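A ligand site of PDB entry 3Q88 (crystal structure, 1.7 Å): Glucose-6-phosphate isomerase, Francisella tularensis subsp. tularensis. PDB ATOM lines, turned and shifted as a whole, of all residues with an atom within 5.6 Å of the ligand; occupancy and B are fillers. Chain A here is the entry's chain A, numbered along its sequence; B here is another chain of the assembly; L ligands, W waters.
N of Phe 204 is in hydrogen-bond range of OG of Ser 201.
The side-chain carboxylate (OE1) of Glu 349 is in hydrogen-bond range of the side-chain amide nitrogen (NE2) of Gln 345 (3.3 Å).
The side-chain hydroxyl of Ser 203 sits close to the backbone NH of Ser 205 (3.2 Å).
The side-chain hydroxyl (OG) of Ser 151 sits close to the backbone carbonyl oxygen (O) of Ala 200 (3.4 Å).
N of Gly 150 sits at hydrogen-bond distance from OE1 of Gln 345, at 3.4 Å.
The backbone carbonyl oxygen (O) of His 380 of chain B is in hydrogen-bond range of the side-chain amide nitrogen (NE2) of Gln 345, 2.7 Å away.
OE1 of Gln 501 lies within hydrogen-bond range of NH2 of Arg 264 (2.8 Å).
O of Gly 263 lies within hydrogen-bond range of OG of Ser 266 (2.7 Å).
Water W6 bridges an oxygen (O6) of the ligand (2.6 Å) and the side-chain amino group of Lys 508 (3.4 Å).
Water W5 lies within hydrogen-bond range of O10 of the ligand, O of Gln 379 of chain B and ND1 of His 380 of chain B.
Water W7 bridges O7 of the ligand (2.7 Å) and OG of Ser 151 (3.5 Å).
Water W1 lies within hydrogen-bond range of O11 of the ligand (2.7 Å), OG1 of Thr 209 (2.7 Å), O of Ala 200 (2.9 Å) and N of Ile 148 (3.2 Å).
Water W3 lies within hydrogen-bond range of O4 of the ligand (2.8 Å), OG1 of Thr 206 (2.9 Å) and NZ of Lys 508 (3.3 Å).
The side-chain hydroxyl (OG) of Ser 201 sits at hydrogen-bond distance from an oxygen (O11) of the ligand (2.5 Å).
An oxygen (O8) of the ligand lies close to the side-chain carboxylate (OE2) of Glu 349 (2.6 Å).
N of Ser 203 lies within hydrogen-bond range of O9 of the ligand, at 2.7 Å.
An oxygen (O9) of the ligand is in hydrogen-bond range of the side-chain hydroxyl of Ser 203, 2.6 Å away.
An oxygen (O11) of the ligand lies within hydrogen-bond range of the side-chain hydroxyl of Thr 206 (2.7 Å).
O3 of the ligand is in hydrogen-bond range of N of Ser 151.
The side-chain hydroxyl of Ser 151 lies within hydrogen-bond range of an oxygen (O7) of the ligand (2.7 Å).
O10 of the ligand is in salt-bridge range of NZ of Lys 508 (2.8 Å).
An oxygen (O2) of the ligand is in hydrogen-bond range of the backbone NH (N) of Gly 150 (2.9 Å).
The side-chain amide nitrogen (NE2) of Gln 345 sits at hydrogen-bond distance from an oxygen (O2) of the ligand (2.9 Å).
O7 of the ligand sits at hydrogen-bond distance from N of Lys 202, at 2.9 Å.
The backbone carbonyl oxygen (O) of His 380 of chain B lies within hydrogen-bond range of an oxygen (O2) of the ligand, at 3.2 Å.
A ring nitrogen (ND1) of His 380 of chain B sits at hydrogen-bond distance from an oxygen (O4) of the ligand (3.0 Å).
O of Ile 148 lies close to O3 of the ligand, 3.5 Å away.
The backbone carbonyl oxygen (O) of Gln 379 of chain B sits close to an oxygen (O8) of the ligand, 3.4 Å away.
Merely in contact with the ligand: Gln 501 (3.4 Å), Val 504 (3.4 Å), Gly 149 (3.5 Å) and Gly 263 (3.9 Å).
Hydrophobic or aromatic side chains within 4 Å of the ligand: Val 504 and His 380 of chain B.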
ATOM      1  N   ILE A 148      12.517  -4.263  34.467  1.00  0.00           N
ATOM      2  CA  ILE A 148      12.006  -5.067  33.336  1.00  0.00           C
ATOM      3  C   ILE A 148      12.854  -4.806  32.106  1.00  0.00           C
ATOM      4  O   ILE A 148      13.537  -3.776  32.028  1.00  0.00           O
ATOM      5  CB  ILE A 148      10.520  -4.759  33.115  1.00  0.00           C
ATOM      6  CG1 ILE A 148       9.769  -5.784  32.265  1.00  0.00           C
ATOM      7  CG2 ILE A 148      10.345  -3.328  32.606  1.00  0.00           C
ATOM      8  CD1 ILE A 148       8.212  -5.653  32.430  1.00  0.00           C
ATOM      9  N   GLY A 149      12.791  -5.759  31.190  1.00  0.00           N
ATOM     10  CA  GLY A 149      13.558  -5.714  29.954  1.00  0.00           C
ATOM     11  C   GLY A 149      15.036  -5.713  30.224  1.00  0.00           C
ATOM     12  O   GLY A 149      15.520  -6.556  30.930  1.00  0.00           O
ATOM     13  N   GLY A 150      15.744  -4.717  29.709  1.00  0.00           N
ATOM     14  CA  GLY A 150      17.160  -4.622  29.923  1.00  0.00           C
ATOM     15  C   GLY A 150      17.611  -4.448  31.372  1.00  0.00           C
ATOM     16  O   GLY A 150      18.742  -4.677  31.742  1.00  0.00           O
ATOM     17  N   SER A 151      16.705  -4.004  32.229  1.00  0.00           N
ATOM     18  CA  SER A 151      16.951  -3.878  33.657  1.00  0.00           C
ATOM     19  C   SER A 151      16.607  -5.149  34.442  1.00  0.00           C
ATOM     20  O   SER A 151      16.673  -5.135  35.665  1.00  0.00           O
ATOM     21  CB  SER A 151      16.147  -2.702  34.195  1.00  0.00           C
ATOM     22  OG  SER A 151      16.632  -1.428  33.594  1.00  0.00           O
ATOM     23  N   ALA A 200      15.930  -0.938  39.507  1.00  0.00           N
ATOM     24  CA  ALA A 200      16.795  -0.830  38.333  1.00  0.00           C
ATOM     25  C   ALA A 200      15.975  -0.157  37.242  1.00  0.00           C
ATOM     26  O   ALA A 200      15.134  -0.803  36.613  1.00  0.00           O
ATOM     27  CB  ALA A 200      17.270  -2.223  37.932  1.00  0.00           C
ATOM     28  N   SER A 201      16.183   1.138  37.046  1.00  0.00           N
ATOM     29  CA  SER A 201      15.374   1.858  36.036  1.00  0.00           C
ATOM     30  C   SER A 201      16.093   3.112  35.530  1.00  0.00           C
ATOM     31  O   SER A 201      16.107   4.104  36.236  1.00  0.00           O
ATOM     32  CB  SER A 201      14.032   2.246  36.638  1.00  0.00           C
ATOM     33  OG  SER A 201      13.159   2.835  35.649  1.00  0.00           O
ATOM     34  N   LYS A 202      16.592   2.996  34.314  1.00  0.00           N
ATOM     35  CA  LYS A 202      17.280   4.148  33.604  1.00  0.00           C
ATOM     36  C   LYS A 202      16.401   5.355  33.687  1.00  0.00           C
ATOM     37  O   LYS A 202      16.788   6.430  34.187  1.00  0.00           O
ATOM     38  CB  LYS A 202      17.628   3.730  32.177  1.00  0.00           C
ATOM     39  CG  LYS A 202      18.405   4.800  31.315  1.00  0.00           C
ATOM     40  CD  LYS A 202      18.883   4.225  29.981  1.00  0.00           C
ATOM     41  CE  LYS A 202      19.692   5.224  29.096  1.00  0.00           C
ATOM     42  NZ  LYS A 202      19.883   4.788  27.628  1.00  0.00           N
ATOM     43  N   SER A 203      15.158   5.187  33.270  1.00  0.00           N
ATOM     44  CA  SER A 203      14.179   6.328  33.245  1.00  0.00           C
ATOM     45  C   SER A 203      13.484   6.709  34.560  1.00  0.00           C
ATOM     46  O   SER A 203      13.040   7.846  34.774  1.00  0.00           O
ATOM     47  CB  SER A 203      13.143   6.025  32.174  1.00  0.00           C
ATOM     48  OG  SER A 203      12.305   4.934  32.591  1.00  0.00           O
ATOM     49  N   PHE A 204      13.317   5.739  35.470  1.00  0.00           N
ATOM     50  CA  PHE A 204      12.513   5.861  36.637  1.00  0.00           C
ATOM     51  C   PHE A 204      11.033   6.138  36.356  1.00  0.00           C
ATOM     52  O   PHE A 204      10.299   6.590  37.226  1.00  0.00           O
ATOM     53  CB  PHE A 204      13.084   6.841  37.686  1.00  0.00           C
ATOM     54  CG  PHE A 204      13.294   6.215  39.029  1.00  0.00           C
ATOM     55  CD1 PHE A 204      14.235   5.194  39.156  1.00  0.00           C
ATOM     56  CD2 PHE A 204      12.508   6.540  40.100  1.00  0.00           C
ATOM     57  CE1 PHE A 204      14.417   4.570  40.363  1.00  0.00           C
ATOM     58  CE2 PHE A 204      12.705   5.909  41.321  1.00  0.00           C
ATOM     59  CZ  PHE A 204      13.651   4.942  41.427  1.00  0.00           C
ATOM     60  N   SER A 205      10.583   5.822  35.149  1.00  0.00           N
ATOM     61  CA  SER A 205       9.176   6.071  34.804  1.00  0.00           C
ATOM     62  C   SER A 205       8.579   4.934  33.945  1.00  0.00           C
ATOM     63  O   SER A 205       7.600   5.148  33.258  1.00  0.00           O
ATOM     64  CB  SER A 205       8.996   7.396  34.064  1.00  0.00           C
ATOM     65  OG  SER A 205       9.767   7.351  32.885  1.00  0.00           O
ATOM     66  N   THR A 206       9.084   3.732  34.092  1.00  0.00           N
ATOM     67  CA  THR A 206       8.541   2.583  33.378  1.00  0.00           C
ATOM     68  C   THR A 206       7.325   2.100  34.165  1.00  0.00           C
ATOM     69  O   THR A 206       7.443   1.837  35.354  1.00  0.00           O
ATOM     70  CB  THR A 206       9.617   1.489  33.265  1.00  0.00           C
ATOM     71  OG1 THR A 206      10.686   1.997  32.471  1.00  0.00           O
ATOM     72  CG2 THR A 206       9.018   0.197  32.592  1.00  0.00           C
ATOM     73  N   THR A 209       7.731  -1.108  36.504  1.00  0.00           N
ATOM     74  CA  THR A 209       8.688  -0.905  37.566  1.00  0.00           C
ATOM     75  C   THR A 209       8.180   0.066  38.585  1.00  0.00           C
ATOM     76  O   THR A 209       8.371  -0.103  39.788  1.00  0.00           O
ATOM     77  CB  THR A 209      10.036  -0.534  36.995  1.00  0.00           C
ATOM     78  OG1 THR A 209      10.438  -1.558  36.072  1.00  0.00           O
ATOM     79  CG2 THR A 209      11.114  -0.382  38.119  1.00  0.00           C
ATOM     80  N   GLY A 263      19.458   0.158  27.361  1.00  0.00           N
ATOM     81  CA  GLY A 263      18.972  -0.867  28.262  1.00  0.00           C
ATOM     82  C   GLY A 263      19.332  -2.277  27.922  1.00  0.00           C
ATOM     83  O   GLY A 263      19.774  -3.070  28.777  1.00  0.00           O
ATOM     84  N   ARG A 264      19.192  -2.644  26.648  1.00  0.00           N
ATOM     85  CA  ARG A 264      19.542  -3.973  26.233  1.00  0.00           C
ATOM     86  C   ARG A 264      21.080  -4.249  26.099  1.00  0.00           C
ATOM     87  O   ARG A 264      21.479  -5.354  25.672  1.00  0.00           O
ATOM     88  CB  ARG A 264      18.792  -4.290  24.916  1.00  0.00           C
ATOM     89  CG  ARG A 264      19.151  -3.371  23.751  1.00  0.00           C
ATOM     90  CD  ARG A 264      18.252  -3.648  22.521  1.00  0.00           C
ATOM     91  NE  ARG A 264      18.427  -2.651  21.449  1.00  0.00           N
ATOM     92  CZ  ARG A 264      17.775  -1.502  21.340  1.00  0.00           C
ATOM     93  NH1 ARG A 264      18.053  -0.697  20.347  1.00  0.00           N
ATOM     94  NH2 ARG A 264      16.816  -1.187  22.235  1.00  0.00           N
ATOM     95  N   SER A 266      23.010  -3.082  28.944  1.00  0.00           N
ATOM     96  CA  SER A 266      23.279  -2.444  30.246  1.00  0.00           C
ATOM     97  C   SER A 266      23.761  -3.393  31.344  1.00  0.00           C
ATOM     98  O   SER A 266      24.103  -2.885  32.405  1.00  0.00           O
ATOM     99  CB  SER A 266      22.069  -1.724  30.760  1.00  0.00           C
ATOM    100  OG  SER A 266      21.000  -2.597  31.140  1.00  0.00           O
ATOM    101  N   ILE A 271      23.609  -1.404  36.470  1.00  0.00           N
ATOM    102  CA  ILE A 271      22.427  -2.304  36.344  1.00  0.00           C
ATOM    103  C   ILE A 271      22.787  -3.766  36.648  1.00  0.00           C
ATOM    104  O   ILE A 271      21.962  -4.535  37.159  1.00  0.00           O
ATOM    105  CB  ILE A 271      21.811  -2.204  34.927  1.00  0.00           C
ATOM    106  CG1 ILE A 271      21.214  -0.844  34.723  1.00  0.00           C
ATOM    107  CG2 ILE A 271      20.830  -3.456  34.685  1.00  0.00           C
ATOM    108  CD1 ILE A 271      19.839  -0.601  35.493  1.00  0.00           C
ATOM    109  N   GLN A 345      16.110 -10.083  22.997  1.00  0.00           N
ATOM    110  CA  GLN A 345      16.055  -8.679  23.268  1.00  0.00           C
ATOM    111  C   GLN A 345      17.174  -7.917  22.553  1.00  0.00           C
ATOM    112  O   GLN A 345      16.922  -6.999  21.754  1.00  0.00           O
ATOM    113  CB  GLN A 345      16.103  -8.369  24.795  1.00  0.00           C
ATOM    114  CG  GLN A 345      16.068  -6.881  24.877  1.00  0.00           C
ATOM    115  CD  GLN A 345      15.839  -6.295  26.198  1.00  0.00           C
ATOM    116  OE1 GLN A 345      15.851  -7.049  27.195  1.00  0.00           O
ATOM    117  NE2 GLN A 345      15.575  -4.883  26.219  1.00  0.00           N
ATOM    118  N   GLU A 349      15.138  -6.224  19.271  1.00  0.00           N
ATOM    119  CA  GLU A 349      14.826  -4.835  19.561  1.00  0.00           C
ATOM    120  C   GLU A 349      15.824  -3.873  18.848  1.00  0.00           C
ATOM    121  O   GLU A 349      15.472  -2.740  18.533  1.00  0.00           O
ATOM    122  CB  GLU A 349      14.848  -4.565  21.050  1.00  0.00           C
ATOM    123  CG  GLU A 349      14.200  -3.265  21.393  1.00  0.00           C
ATOM    124  CD  GLU A 349      13.948  -3.095  22.874  1.00  0.00           C
ATOM    125  OE1 GLU A 349      14.923  -2.932  23.622  1.00  0.00           O
ATOM    126  OE2 GLU A 349      12.763  -3.100  23.275  1.00  0.00           O
ATOM    127  N   GLN A 501      14.605   2.634  19.657  1.00  0.00           N
ATOM    128  CA  GLN A 501      13.479   1.699  19.795  1.00  0.00           C
ATOM    129  C   GLN A 501      12.186   2.451  19.825  1.00  0.00           C
ATOM    130  O   GLN A 501      11.420   2.403  20.800  1.00  0.00           O
ATOM    131  CB  GLN A 501      13.617   0.830  21.060  1.00  0.00           C
ATOM    132  CG  GLN A 501      13.831   1.602  22.355  1.00  0.00           C
ATOM    133  CD  GLN A 501      15.223   2.188  22.534  1.00  0.00           C
ATOM    134  OE1 GLN A 501      16.243   1.553  22.173  1.00  0.00           O
ATOM    135  NE2 GLN A 501      15.283   3.403  23.124  1.00  0.00           N
ATOM    136  N   VAL A 504       8.065   0.924  20.326  1.00  0.00           N
ATOM    137  CA  VAL A 504       7.386   0.565  21.582  1.00  0.00           C
ATOM    138  C   VAL A 504       6.562   1.704  22.136  1.00  0.00           C
ATOM    139  O   VAL A 504       5.789   1.503  23.051  1.00  0.00           O
ATOM    140  CB  VAL A 504       8.389   0.057  22.634  1.00  0.00           C
ATOM    141  CG1 VAL A 504       9.203  -1.187  22.004  1.00  0.00           C
ATOM    142  CG2 VAL A 504       9.316   1.167  23.139  1.00  0.00           C
ATOM    143  N   LYS A 508       2.667   1.973  24.706  1.00  0.00           N
ATOM    144  CA  LYS A 508       2.666   2.596  26.047  1.00  0.00           C
ATOM    145  C   LYS A 508       1.569   3.676  26.174  1.00  0.00           C
ATOM    146  O   LYS A 508       0.868   3.690  27.184  1.00  0.00           O
ATOM    147  CB  LYS A 508       4.052   3.178  26.394  1.00  0.00           C
ATOM    148  CG  LYS A 508       5.153   2.138  26.531  1.00  0.00           C
ATOM    149  CD  LYS A 508       6.556   2.772  26.732  1.00  0.00           C
ATOM    150  CE  LYS A 508       7.627   1.710  26.784  1.00  0.00           C
ATOM    151  NZ  LYS A 508       8.984   2.317  26.934  1.00  0.00           N
ATOM    152  N   GLN B 379       7.250  -7.002  25.724  1.00  0.00           N
ATOM    153  CA  GLN B 379       7.111  -5.653  25.204  1.00  0.00           C
ATOM    154  C   GLN B 379       8.421  -4.886  25.244  1.00  0.00           C
ATOM    155  O   GLN B 379       8.601  -3.937  24.470  1.00  0.00           O
ATOM    156  CB  GLN B 379       6.074  -4.836  25.977  1.00  0.00           C
ATOM    157  CG  GLN B 379       4.619  -5.375  25.855  1.00  0.00           C
ATOM    158  CD  GLN B 379       3.621  -4.811  26.837  1.00  0.00           C
ATOM    159  OE1 GLN B 379       2.609  -5.459  27.058  1.00  0.00           O
ATOM    160  NE2 GLN B 379       3.862  -3.584  27.397  1.00  0.00           N
ATOM    161  N   HIS B 380       9.305  -5.287  26.191  1.00  0.00           N
ATOM    162  CA  HIS B 380      10.606  -4.638  26.382  1.00  0.00           C
ATOM    163  C   HIS B 380      11.723  -5.472  25.845  1.00  0.00           C
ATOM    164  O   HIS B 380      12.902  -5.286  26.228  1.00  0.00           O
ATOM    165  CB  HIS B 380      10.856  -4.372  27.872  1.00  0.00           C
ATOM    166  CG  HIS B 380       9.731  -3.652  28.547  1.00  0.00           C
ATOM    167  ND1 HIS B 380       9.724  -2.269  28.767  1.00  0.00           N
ATOM    168  CD2 HIS B 380       8.545  -4.098  29.016  1.00  0.00           C
ATOM    169  CE1 HIS B 380       8.588  -1.938  29.344  1.00  0.00           C
ATOM    170  NE2 HIS B 380       7.855  -3.030  29.532  1.00  0.00           N
ATOM    171  N   ALA B 381      11.375  -6.460  25.026  1.00  0.00           N
ATOM    172  CA  ALA B 381      12.360  -7.326  24.409  1.00  0.00           C
ATOM    173  C   ALA B 381      12.258  -7.468  22.930  1.00  0.00           C
ATOM    174  O   ALA B 381      13.214  -7.131  22.227  1.00  0.00           O
ATOM    175  CB  ALA B 381      12.323  -8.732  25.081  1.00  0.00           C
HETATM  176  P1  LIG L   1      13.962   1.494  32.498  1.00  0.00           P
HETATM  177  C1  LIG L   1      13.177  -0.854  27.842  1.00  0.00           C
HETATM  178  O1  LIG L   1      12.413  -1.488  26.856  1.00  0.00           O
HETATM  179  C2  LIG L   1      14.492  -1.540  28.109  1.00  0.00           C
HETATM  180  O2  LIG L   1      14.326  -2.961  27.965  1.00  0.00           O
HETATM  181  C3  LIG L   1      14.713  -1.118  29.492  1.00  0.00           C
HETATM  182  O3  LIG L   1      15.726  -1.840  30.151  1.00  0.00           O
HETATM  183  C4  LIG L   1      13.305  -1.356  30.047  1.00  0.00           C
HETATM  184  O4  LIG L   1      12.405  -0.854  29.074  1.00  0.00           O
HETATM  185  C5  LIG L   1      13.118  -0.699  31.356  1.00  0.00           C
HETATM  186  O5  LIG L   1      13.398   0.716  31.218  1.00  0.00           O
HETATM  187  P2  LIG L   1      11.557  -0.604  25.820  1.00  0.00           P
HETATM  188  O6  LIG L   1      12.495   0.443  25.264  1.00  0.00           O
HETATM  189  O7  LIG L   1      15.345   0.848  32.801  1.00  0.00           O
HETATM  190  O8  LIG L   1      11.189  -1.688  24.741  1.00  0.00           O
HETATM  191  O9  LIG L   1      14.063   3.017  32.091  1.00  0.00           O
HETATM  192  O10 LIG L   1      10.309  -0.073  26.535  1.00  0.00           O
HETATM  193  O11 LIG L   1      12.956   1.276  33.666  1.00  0.00           O
HETATM  194  O   HOH W   1      12.855  -1.102  34.914  1.00  0.00           O
HETATM  195  O   HOH W   2      14.436   3.628  29.550  1.00  0.00           O
HETATM  196  O   HOH W   3      10.527   1.184  29.681  1.00  0.00           O
HETATM  197  O   HOH W   4      16.306   1.732  28.233  1.00  0.00           O
HETATM  198  O   HOH W   5       8.258  -1.532  25.904  1.00  0.00           O
HETATM  199  O   HOH W   6      12.097   2.958  25.689  1.00  0.00           O
HETATM  200  O   HOH W   7      17.064   0.562  30.784  1.00  0.00           O
